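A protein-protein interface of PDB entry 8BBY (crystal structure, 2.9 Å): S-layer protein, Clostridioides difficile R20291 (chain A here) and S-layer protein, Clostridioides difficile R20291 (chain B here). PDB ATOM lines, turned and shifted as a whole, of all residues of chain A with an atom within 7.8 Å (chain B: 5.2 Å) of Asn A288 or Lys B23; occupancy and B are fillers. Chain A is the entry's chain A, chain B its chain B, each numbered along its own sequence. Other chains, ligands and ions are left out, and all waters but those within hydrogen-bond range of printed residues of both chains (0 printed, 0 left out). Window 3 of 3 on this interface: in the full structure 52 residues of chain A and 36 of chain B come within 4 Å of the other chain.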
ATOM      1  N   ILE A 258      25.687 -19.631  18.683  1.00  0.00           N
ATOM      2  CA  ILE A 258      26.219 -20.286  17.495  1.00  0.00           C
ATOM      3  C   ILE A 258      26.252 -19.353  16.293  1.00  0.00           C
ATOM      4  O   ILE A 258      26.945 -19.641  15.310  1.00  0.00           O
ATOM      5  CB  ILE A 258      25.405 -21.551  17.178  1.00  0.00           C
ATOM      6  CG1 ILE A 258      23.938 -21.190  16.964  1.00  0.00           C
ATOM      7  CG2 ILE A 258      25.539 -22.564  18.306  1.00  0.00           C
ATOM      8  CD1 ILE A 258      23.037 -22.383  16.900  1.00  0.00           C
ATOM      9  N   ASN A 281      18.635 -36.052  19.329  1.00  0.00           N
ATOM     10  CA  ASN A 281      17.764 -36.527  18.258  1.00  0.00           C
ATOM     11  C   ASN A 281      16.377 -35.903  18.360  1.00  0.00           C
ATOM     12  O   ASN A 281      15.902 -35.258  17.418  1.00  0.00           O
ATOM     13  CB  ASN A 281      17.673 -38.053  18.290  1.00  0.00           C
ATOM     14  CG  ASN A 281      18.901 -38.722  17.708  1.00  0.00           C
ATOM     15  OD1 ASN A 281      19.709 -38.083  17.036  1.00  0.00           O
ATOM     16  ND2 ASN A 281      19.045 -40.018  17.960  1.00  0.00           N
ATOM     17  N   THR A 282      15.705 -36.091  19.500  1.00  0.00           N
ATOM     18  CA  THR A 282      14.365 -35.539  19.665  1.00  0.00           C
ATOM     19  C   THR A 282      14.363 -34.016  19.615  1.00  0.00           C
ATOM     20  O   THR A 282      13.330 -33.420  19.288  1.00  0.00           O
ATOM     21  CB  THR A 282      13.742 -36.033  20.977  1.00  0.00           C
ATOM     22  OG1 THR A 282      12.313 -35.996  20.874  1.00  0.00           O
ATOM     23  CG2 THR A 282      14.184 -35.179  22.159  1.00  0.00           C
ATOM     24  N   LEU A 283      15.492 -33.377  19.927  1.00  0.00           N
ATOM     25  CA  LEU A 283      15.590 -31.932  19.759  1.00  0.00           C
ATOM     26  C   LEU A 283      15.580 -31.554  18.284  1.00  0.00           C
ATOM     27  O   LEU A 283      14.913 -30.591  17.888  1.00  0.00           O
ATOM     28  CB  LEU A 283      16.851 -31.410  20.445  1.00  0.00           C
ATOM     29  CG  LEU A 283      17.133 -29.914  20.320  1.00  0.00           C
ATOM     30  CD1 LEU A 283      15.941 -29.115  20.816  1.00  0.00           C
ATOM     31  CD2 LEU A 283      18.391 -29.541  21.089  1.00  0.00           C
ATOM     32  N   TYR A 284      16.311 -32.306  17.458  1.00  0.00           N
ATOM     33  CA  TYR A 284      16.334 -32.034  16.025  1.00  0.00           C
ATOM     34  C   TYR A 284      14.966 -32.268  15.395  1.00  0.00           C
ATOM     35  O   TYR A 284      14.540 -31.507  14.517  1.00  0.00           O
ATOM     36  CB  TYR A 284      17.406 -32.898  15.349  1.00  0.00           C
ATOM     37  CG  TYR A 284      17.293 -32.996  13.839  1.00  0.00           C
ATOM     38  CD1 TYR A 284      16.481 -33.953  13.238  1.00  0.00           C
ATOM     39  CD2 TYR A 284      17.998 -32.128  13.017  1.00  0.00           C
ATOM     40  CE1 TYR A 284      16.378 -34.041  11.863  1.00  0.00           C
ATOM     41  CE2 TYR A 284      17.901 -32.209  11.642  1.00  0.00           C
ATOM     42  CZ  TYR A 284      17.090 -33.166  11.070  1.00  0.00           C
ATOM     43  OH  TYR A 284      16.992 -33.248   9.699  1.00  0.00           O
ATOM     44  N   ARG A 285      14.268 -33.325  15.821  1.00  0.00           N
ATOM     45  CA  ARG A 285      12.991 -33.671  15.204  1.00  0.00           C
ATOM     46  C   ARG A 285      11.957 -32.568  15.403  1.00  0.00           C
ATOM     47  O   ARG A 285      11.205 -32.239  14.478  1.00  0.00           O
ATOM     48  CB  ARG A 285      12.482 -35.000  15.764  1.00  0.00           C
ATOM     49  CG  ARG A 285      13.300 -36.204  15.320  1.00  0.00           C
ATOM     50  CD  ARG A 285      13.229 -37.339  16.330  1.00  0.00           C
ATOM     51  NE  ARG A 285      12.082 -37.218  17.223  1.00  0.00           N
ATOM     52  CZ  ARG A 285      11.984 -37.824  18.398  1.00  0.00           C
ATOM     53  NH1 ARG A 285      12.948 -38.605  18.856  1.00  0.00           N
ATOM     54  NH2 ARG A 285      10.890 -37.640  19.133  1.00  0.00           N
ATOM     55  N   VAL A 286      11.902 -31.989  16.605  1.00  0.00           N
ATOM     56  CA  VAL A 286      11.007 -30.858  16.840  1.00  0.00           C
ATOM     57  C   VAL A 286      11.430 -29.665  15.994  1.00  0.00           C
ATOM     58  O   VAL A 286      10.591 -28.953  15.428  1.00  0.00           O
ATOM     59  CB  VAL A 286      10.972 -30.507  18.341  1.00  0.00           C
ATOM     60  CG1 VAL A 286      10.211 -29.210  18.569  1.00  0.00           C
ATOM     61  CG2 VAL A 286      10.352 -31.645  19.137  1.00  0.00           C
ATOM     62  N   LEU A 287      12.740 -29.430  15.894  1.00  0.00           N
ATOM     63  CA  LEU A 287      13.244 -28.311  15.104  1.00  0.00           C
ATOM     64  C   LEU A 287      12.949 -28.491  13.621  1.00  0.00           C
ATOM     65  O   LEU A 287      12.608 -27.525  12.929  1.00  0.00           O
ATOM     66  CB  LEU A 287      14.743 -28.151  15.337  1.00  0.00           C
ATOM     67  CG  LEU A 287      15.080 -27.613  16.722  1.00  0.00           C
ATOM     68  CD1 LEU A 287      16.548 -27.829  17.051  1.00  0.00           C
ATOM     69  CD2 LEU A 287      14.707 -26.146  16.780  1.00  0.00           C
ATOM     70  N   ASN A 288      13.079 -29.718  13.112  1.00  0.00           N
ATOM     71  CA  ASN A 288      12.804 -29.972  11.704  1.00  0.00           C
ATOM     72  C   ASN A 288      11.325 -29.821  11.368  1.00  0.00           C
ATOM     73  O   ASN A 288      10.980 -29.674  10.191  1.00  0.00           O
ATOM     74  CB  ASN A 288      13.291 -31.373  11.323  1.00  0.00           C
ATOM     75  CG  ASN A 288      13.124 -31.670   9.845  1.00  0.00           C
ATOM     76  OD1 ASN A 288      13.649 -30.953   8.993  1.00  0.00           O
ATOM     77  ND2 ASN A 288      12.390 -32.732   9.533  1.00  0.00           N
ATOM     78  N   GLY A 289      10.450 -29.834  12.372  1.00  0.00           N
ATOM     79  CA  GLY A 289       9.024 -29.723  12.158  1.00  0.00           C
ATOM     80  C   GLY A 289       8.269 -31.033  12.189  1.00  0.00           C
ATOM     81  O   GLY A 289       7.044 -31.024  12.019  1.00  0.00           O
ATOM     82  N   ASP A 290       8.958 -32.157  12.400  1.00  0.00           N
ATOM     83  CA  ASP A 290       8.278 -33.446  12.447  1.00  0.00           C
ATOM     84  C   ASP A 290       7.362 -33.560  13.658  1.00  0.00           C
ATOM     85  O   ASP A 290       6.394 -34.328  13.630  1.00  0.00           O
ATOM     86  CB  ASP A 290       9.303 -34.581  12.453  1.00  0.00           C
ATOM     87  CG  ASP A 290      10.295 -34.477  11.313  1.00  0.00           C
ATOM     88  OD1 ASP A 290       9.965 -34.920  10.192  1.00  0.00           O
ATOM     89  OD2 ASP A 290      11.406 -33.954  11.537  1.00  0.00           O
ATOM     90  N   GLU A 291       7.646 -32.812  14.721  1.00  0.00           N
ATOM     91  CA  GLU A 291       6.847 -32.842  15.936  1.00  0.00           C
ATOM     92  C   GLU A 291       6.410 -31.430  16.292  1.00  0.00           C
ATOM     93  O   GLU A 291       7.199 -30.484  16.198  1.00  0.00           O
ATOM     94  CB  GLU A 291       7.628 -33.452  17.107  1.00  0.00           C
ATOM     95  CG  GLU A 291       8.085 -34.882  16.875  1.00  0.00           C
ATOM     96  CD  GLU A 291       8.916 -35.419  18.024  1.00  0.00           C
ATOM     97  OE1 GLU A 291       9.997 -34.855  18.291  1.00  0.00           O
ATOM     98  OE2 GLU A 291       8.488 -36.405  18.660  1.00  0.00           O
ATOM     99  N   VAL A 298      11.571 -25.453  21.872  1.00  0.00           N
ATOM    100  CA  VAL A 298      12.072 -24.278  21.168  1.00  0.00           C
ATOM    101  C   VAL A 298      11.329 -23.074  21.736  1.00  0.00           C
ATOM    102  O   VAL A 298      10.131 -22.903  21.495  1.00  0.00           O
ATOM    103  CB  VAL A 298      11.870 -24.400  19.653  1.00  0.00           C
ATOM    104  CG1 VAL A 298      12.769 -23.417  18.912  1.00  0.00           C
ATOM    105  CG2 VAL A 298      12.117 -25.832  19.200  1.00  0.00           C
ATOM    106  N   TYR A 305      15.701 -17.749  19.180  1.00  0.00           N
ATOM    107  CA  TYR A 305      15.293 -19.124  19.431  1.00  0.00           C
ATOM    108  C   TYR A 305      16.409 -19.823  20.195  1.00  0.00           C
ATOM    109  O   TYR A 305      17.578 -19.739  19.806  1.00  0.00           O
ATOM    110  CB  TYR A 305      14.998 -19.856  18.121  1.00  0.00           C
ATOM    111  CG  TYR A 305      13.799 -19.316  17.377  1.00  0.00           C
ATOM    112  CD1 TYR A 305      12.509 -19.538  17.841  1.00  0.00           C
ATOM    113  CD2 TYR A 305      13.956 -18.580  16.211  1.00  0.00           C
ATOM    114  CE1 TYR A 305      11.409 -19.046  17.163  1.00  0.00           C
ATOM    115  CE2 TYR A 305      12.865 -18.082  15.526  1.00  0.00           C
ATOM    116  CZ  TYR A 305      11.594 -18.318  16.006  1.00  0.00           C
ATOM    117  OH  TYR A 305      10.505 -17.823  15.326  1.00  0.00           O
ATOM    118  N   LYS B  21      17.518 -17.752  13.840  1.00  0.00           N
ATOM    119  CA  LYS B  21      16.674 -18.614  13.026  1.00  0.00           C
ATOM    120  C   LYS B  21      16.702 -20.032  13.577  1.00  0.00           C
ATOM    121  O   LYS B  21      17.756 -20.526  13.992  1.00  0.00           O
ATOM    122  CB  LYS B  21      17.133 -18.608  11.564  1.00  0.00           C
ATOM    123  CG  LYS B  21      16.164 -19.272  10.598  1.00  0.00           C
ATOM    124  CD  LYS B  21      14.770 -18.679  10.701  1.00  0.00           C
ATOM    125  CE  LYS B  21      13.736 -19.756  10.974  1.00  0.00           C
ATOM    126  NZ  LYS B  21      12.391 -19.187  11.253  1.00  0.00           N
ATOM    127  N   LYS B  22      15.538 -20.683  13.580  1.00  0.00           N
ATOM    128  CA  LYS B  22      15.443 -22.047  14.087  1.00  0.00           C
ATOM    129  C   LYS B  22      16.119 -23.061  13.171  1.00  0.00           C
ATOM    130  O   LYS B  22      16.495 -24.142  13.637  1.00  0.00           O
ATOM    131  CB  LYS B  22      13.977 -22.427  14.300  1.00  0.00           C
ATOM    132  CG  LYS B  22      13.228 -22.790  13.025  1.00  0.00           C
ATOM    133  CD  LYS B  22      11.891 -23.458  13.325  1.00  0.00           C
ATOM    134  CE  LYS B  22      11.318 -22.998  14.659  1.00  0.00           C
ATOM    135  NZ  LYS B  22      10.048 -23.698  14.996  1.00  0.00           N
ATOM    136  N   LYS B  23      16.279 -22.743  11.885  1.00  0.00           N
ATOM    137  CA  LYS B  23      16.959 -23.665  10.982  1.00  0.00           C
ATOM    138  C   LYS B  23      18.462 -23.672  11.220  1.00  0.00           C
ATOM    139  O   LYS B  23      19.126 -24.682  10.955  1.00  0.00           O
ATOM    140  CB  LYS B  23      16.650 -23.306   9.527  1.00  0.00           C
ATOM    141  CG  LYS B  23      15.200 -23.538   9.117  1.00  0.00           C
ATOM    142  CD  LYS B  23      14.576 -24.699   9.881  1.00  0.00           C
ATOM    143  CE  LYS B  23      13.069 -24.742   9.695  1.00  0.00           C
ATOM    144  NZ  LYS B  23      12.561 -26.138   9.616  1.00  0.00           N
ATOM    145  N   ASP B  24      19.017 -22.562  11.711  1.00  0.00           N
ATOM    146  CA  ASP B  24      20.447 -22.508  11.990  1.00  0.00           C
ATOM    147  C   ASP B  24      20.817 -23.426  13.149  1.00  0.00           C
ATOM    148  O   ASP B  24      21.766 -24.213  13.052  1.00  0.00           O
ATOM    149  CB  ASP B  24      20.871 -21.068  12.285  1.00  0.00           C
ATOM    150  CG  ASP B  24      21.257 -20.307  11.032  1.00  0.00           C
ATOM    151  OD1 ASP B  24      20.836 -20.718   9.929  1.00  0.00           O
ATOM    152  OD2 ASP B  24      21.983 -19.297  11.148  1.00  0.00           O
ATOM    153  N   LEU B  25      20.078 -23.343  14.257  1.00  0.00           N
ATOM    154  CA  LEU B  25      20.375 -24.191  15.403  1.00  0.00           C
ATOM    155  C   LEU B  25      19.933 -25.632  15.188  1.00  0.00           C
ATOM    156  O   LEU B  25      20.466 -26.534  15.843  1.00  0.00           O
ATOM    157  CB  LEU B  25      19.741 -23.616  16.675  1.00  0.00           C
ATOM    158  CG  LEU B  25      18.237 -23.379  16.778  1.00  0.00           C
ATOM    159  CD1 LEU B  25      17.623 -24.467  17.620  1.00  0.00           C
ATOM    160  CD2 LEU B  25      17.944 -22.020  17.382  1.00  0.00           C
ATOM    161  N   LYS B  26      18.975 -25.868  14.287  1.00  0.00           N
ATOM    162  CA  LYS B  26      18.680 -27.235  13.873  1.00  0.00           C
ATOM    163  C   LYS B  26      19.878 -27.855  13.164  1.00  0.00           C
ATOM    164  O   LYS B  26      20.194 -29.033  13.370  1.00  0.00           O
ATOM    165  CB  LYS B  26      17.444 -27.254  12.972  1.00  0.00           C
ATOM    166  CG  LYS B  26      17.263 -28.536  12.174  1.00  0.00           C
ATOM    167  CD  LYS B  26      16.270 -28.343  11.038  1.00  0.00           C
ATOM    168  CE  LYS B  26      16.665 -29.149   9.809  1.00  0.00           C
ATOM    169  NZ  LYS B  26      15.713 -28.944   8.683  1.00  0.00           N
ATOM    170  N   ASP B  27      20.562 -27.071  12.326  1.00  0.00           N
ATOM    171  CA  ASP B  27      21.773 -27.556  11.673  1.00  0.00           C
ATOM    172  C   ASP B  27      22.900 -27.763  12.676  1.00  0.00           C
ATOM    173  O   ASP B  27      23.674 -28.720  12.558  1.00  0.00           O
ATOM    174  CB  ASP B  27      22.203 -26.582  10.577  1.00  0.00           C
ATOM    175  CG  ASP B  27      21.359 -26.703   9.324  1.00  0.00           C
ATOM    176  OD1 ASP B  27      20.517 -27.624   9.260  1.00  0.00           O
ATOM    177  OD2 ASP B  27      21.538 -25.879   8.403  1.00  0.00           O
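The side-chain carboxylate (OD2) of Asp A290 is in hydrogen-bond range of the side-chain amide nitrogen (ND2) of Asn A288, at 2.5 Å.
Printed residues of chain A that touch a printed residue of chain B: Ile A258, Tyr A284, Leu A287, Asn A288 and Tyr A305. Hydrophobic or aromatic side chains of chain A within 4 Å of the printed part of chain B: Ile A258, Tyr A284, Leu A287 and Tyr A305. Along chain A the printed residues that touch a printed residue of chain B span positions 258 to 305. Printed residues of chain B that touch a printed residue of chain A: Lys B22, Lys B23, Leu B25 and Lys B26. Hydrophobic or aromatic side chains of chain B within 4 Å of the printed part of chain A: Leu B25. Along chain B the printed residues that touch a printed residue of chain A span positions 22 to 26. Among the printed residues, 9 pairs touch across the chains.
Among the printed residues, pairs that only touch across the chains: Ile A258 with Leu B25 (3.5 Å), Tyr A284 with Lys B26 (3.8 Å), Leu A287 with Lys B23 (3.6 Å), Leu A287 with Leu B25 (3.5 Å), Leu A287 with Lys B26 (3.7 Å), Asn A288 with Lys B23 (3.9 Å), Tyr A305 with Lys B22 (3.7 Å) and Tyr A305 with Leu B25 (3.3 Å).
The side-chain amide oxygen (OD1) of Asn A288 is in hydrogen-bond range of the side-chain amino group (NZ) of Lys B26, 2.9 Å away.
Of chain B, only Lys B23 and Lys B26 come within 4 Å of Asn A288. Lys B23 touches just these residues of chain A: Leu A287 (3.6 Å) and Asn A288 (3.9 Å). Printed residues of chain B within 4 Å of Tyr A284: Lys B26 (3.8 Å). Of the printed residues of chain A, Lys B26 touches Tyr A284 (3.8 Å), Leu A287 (3.7 Å) and Asn A288 (2.9 Å). The nearest residue of chain A that does not touch Lys B23 is Gly A289 (5.1 Å).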
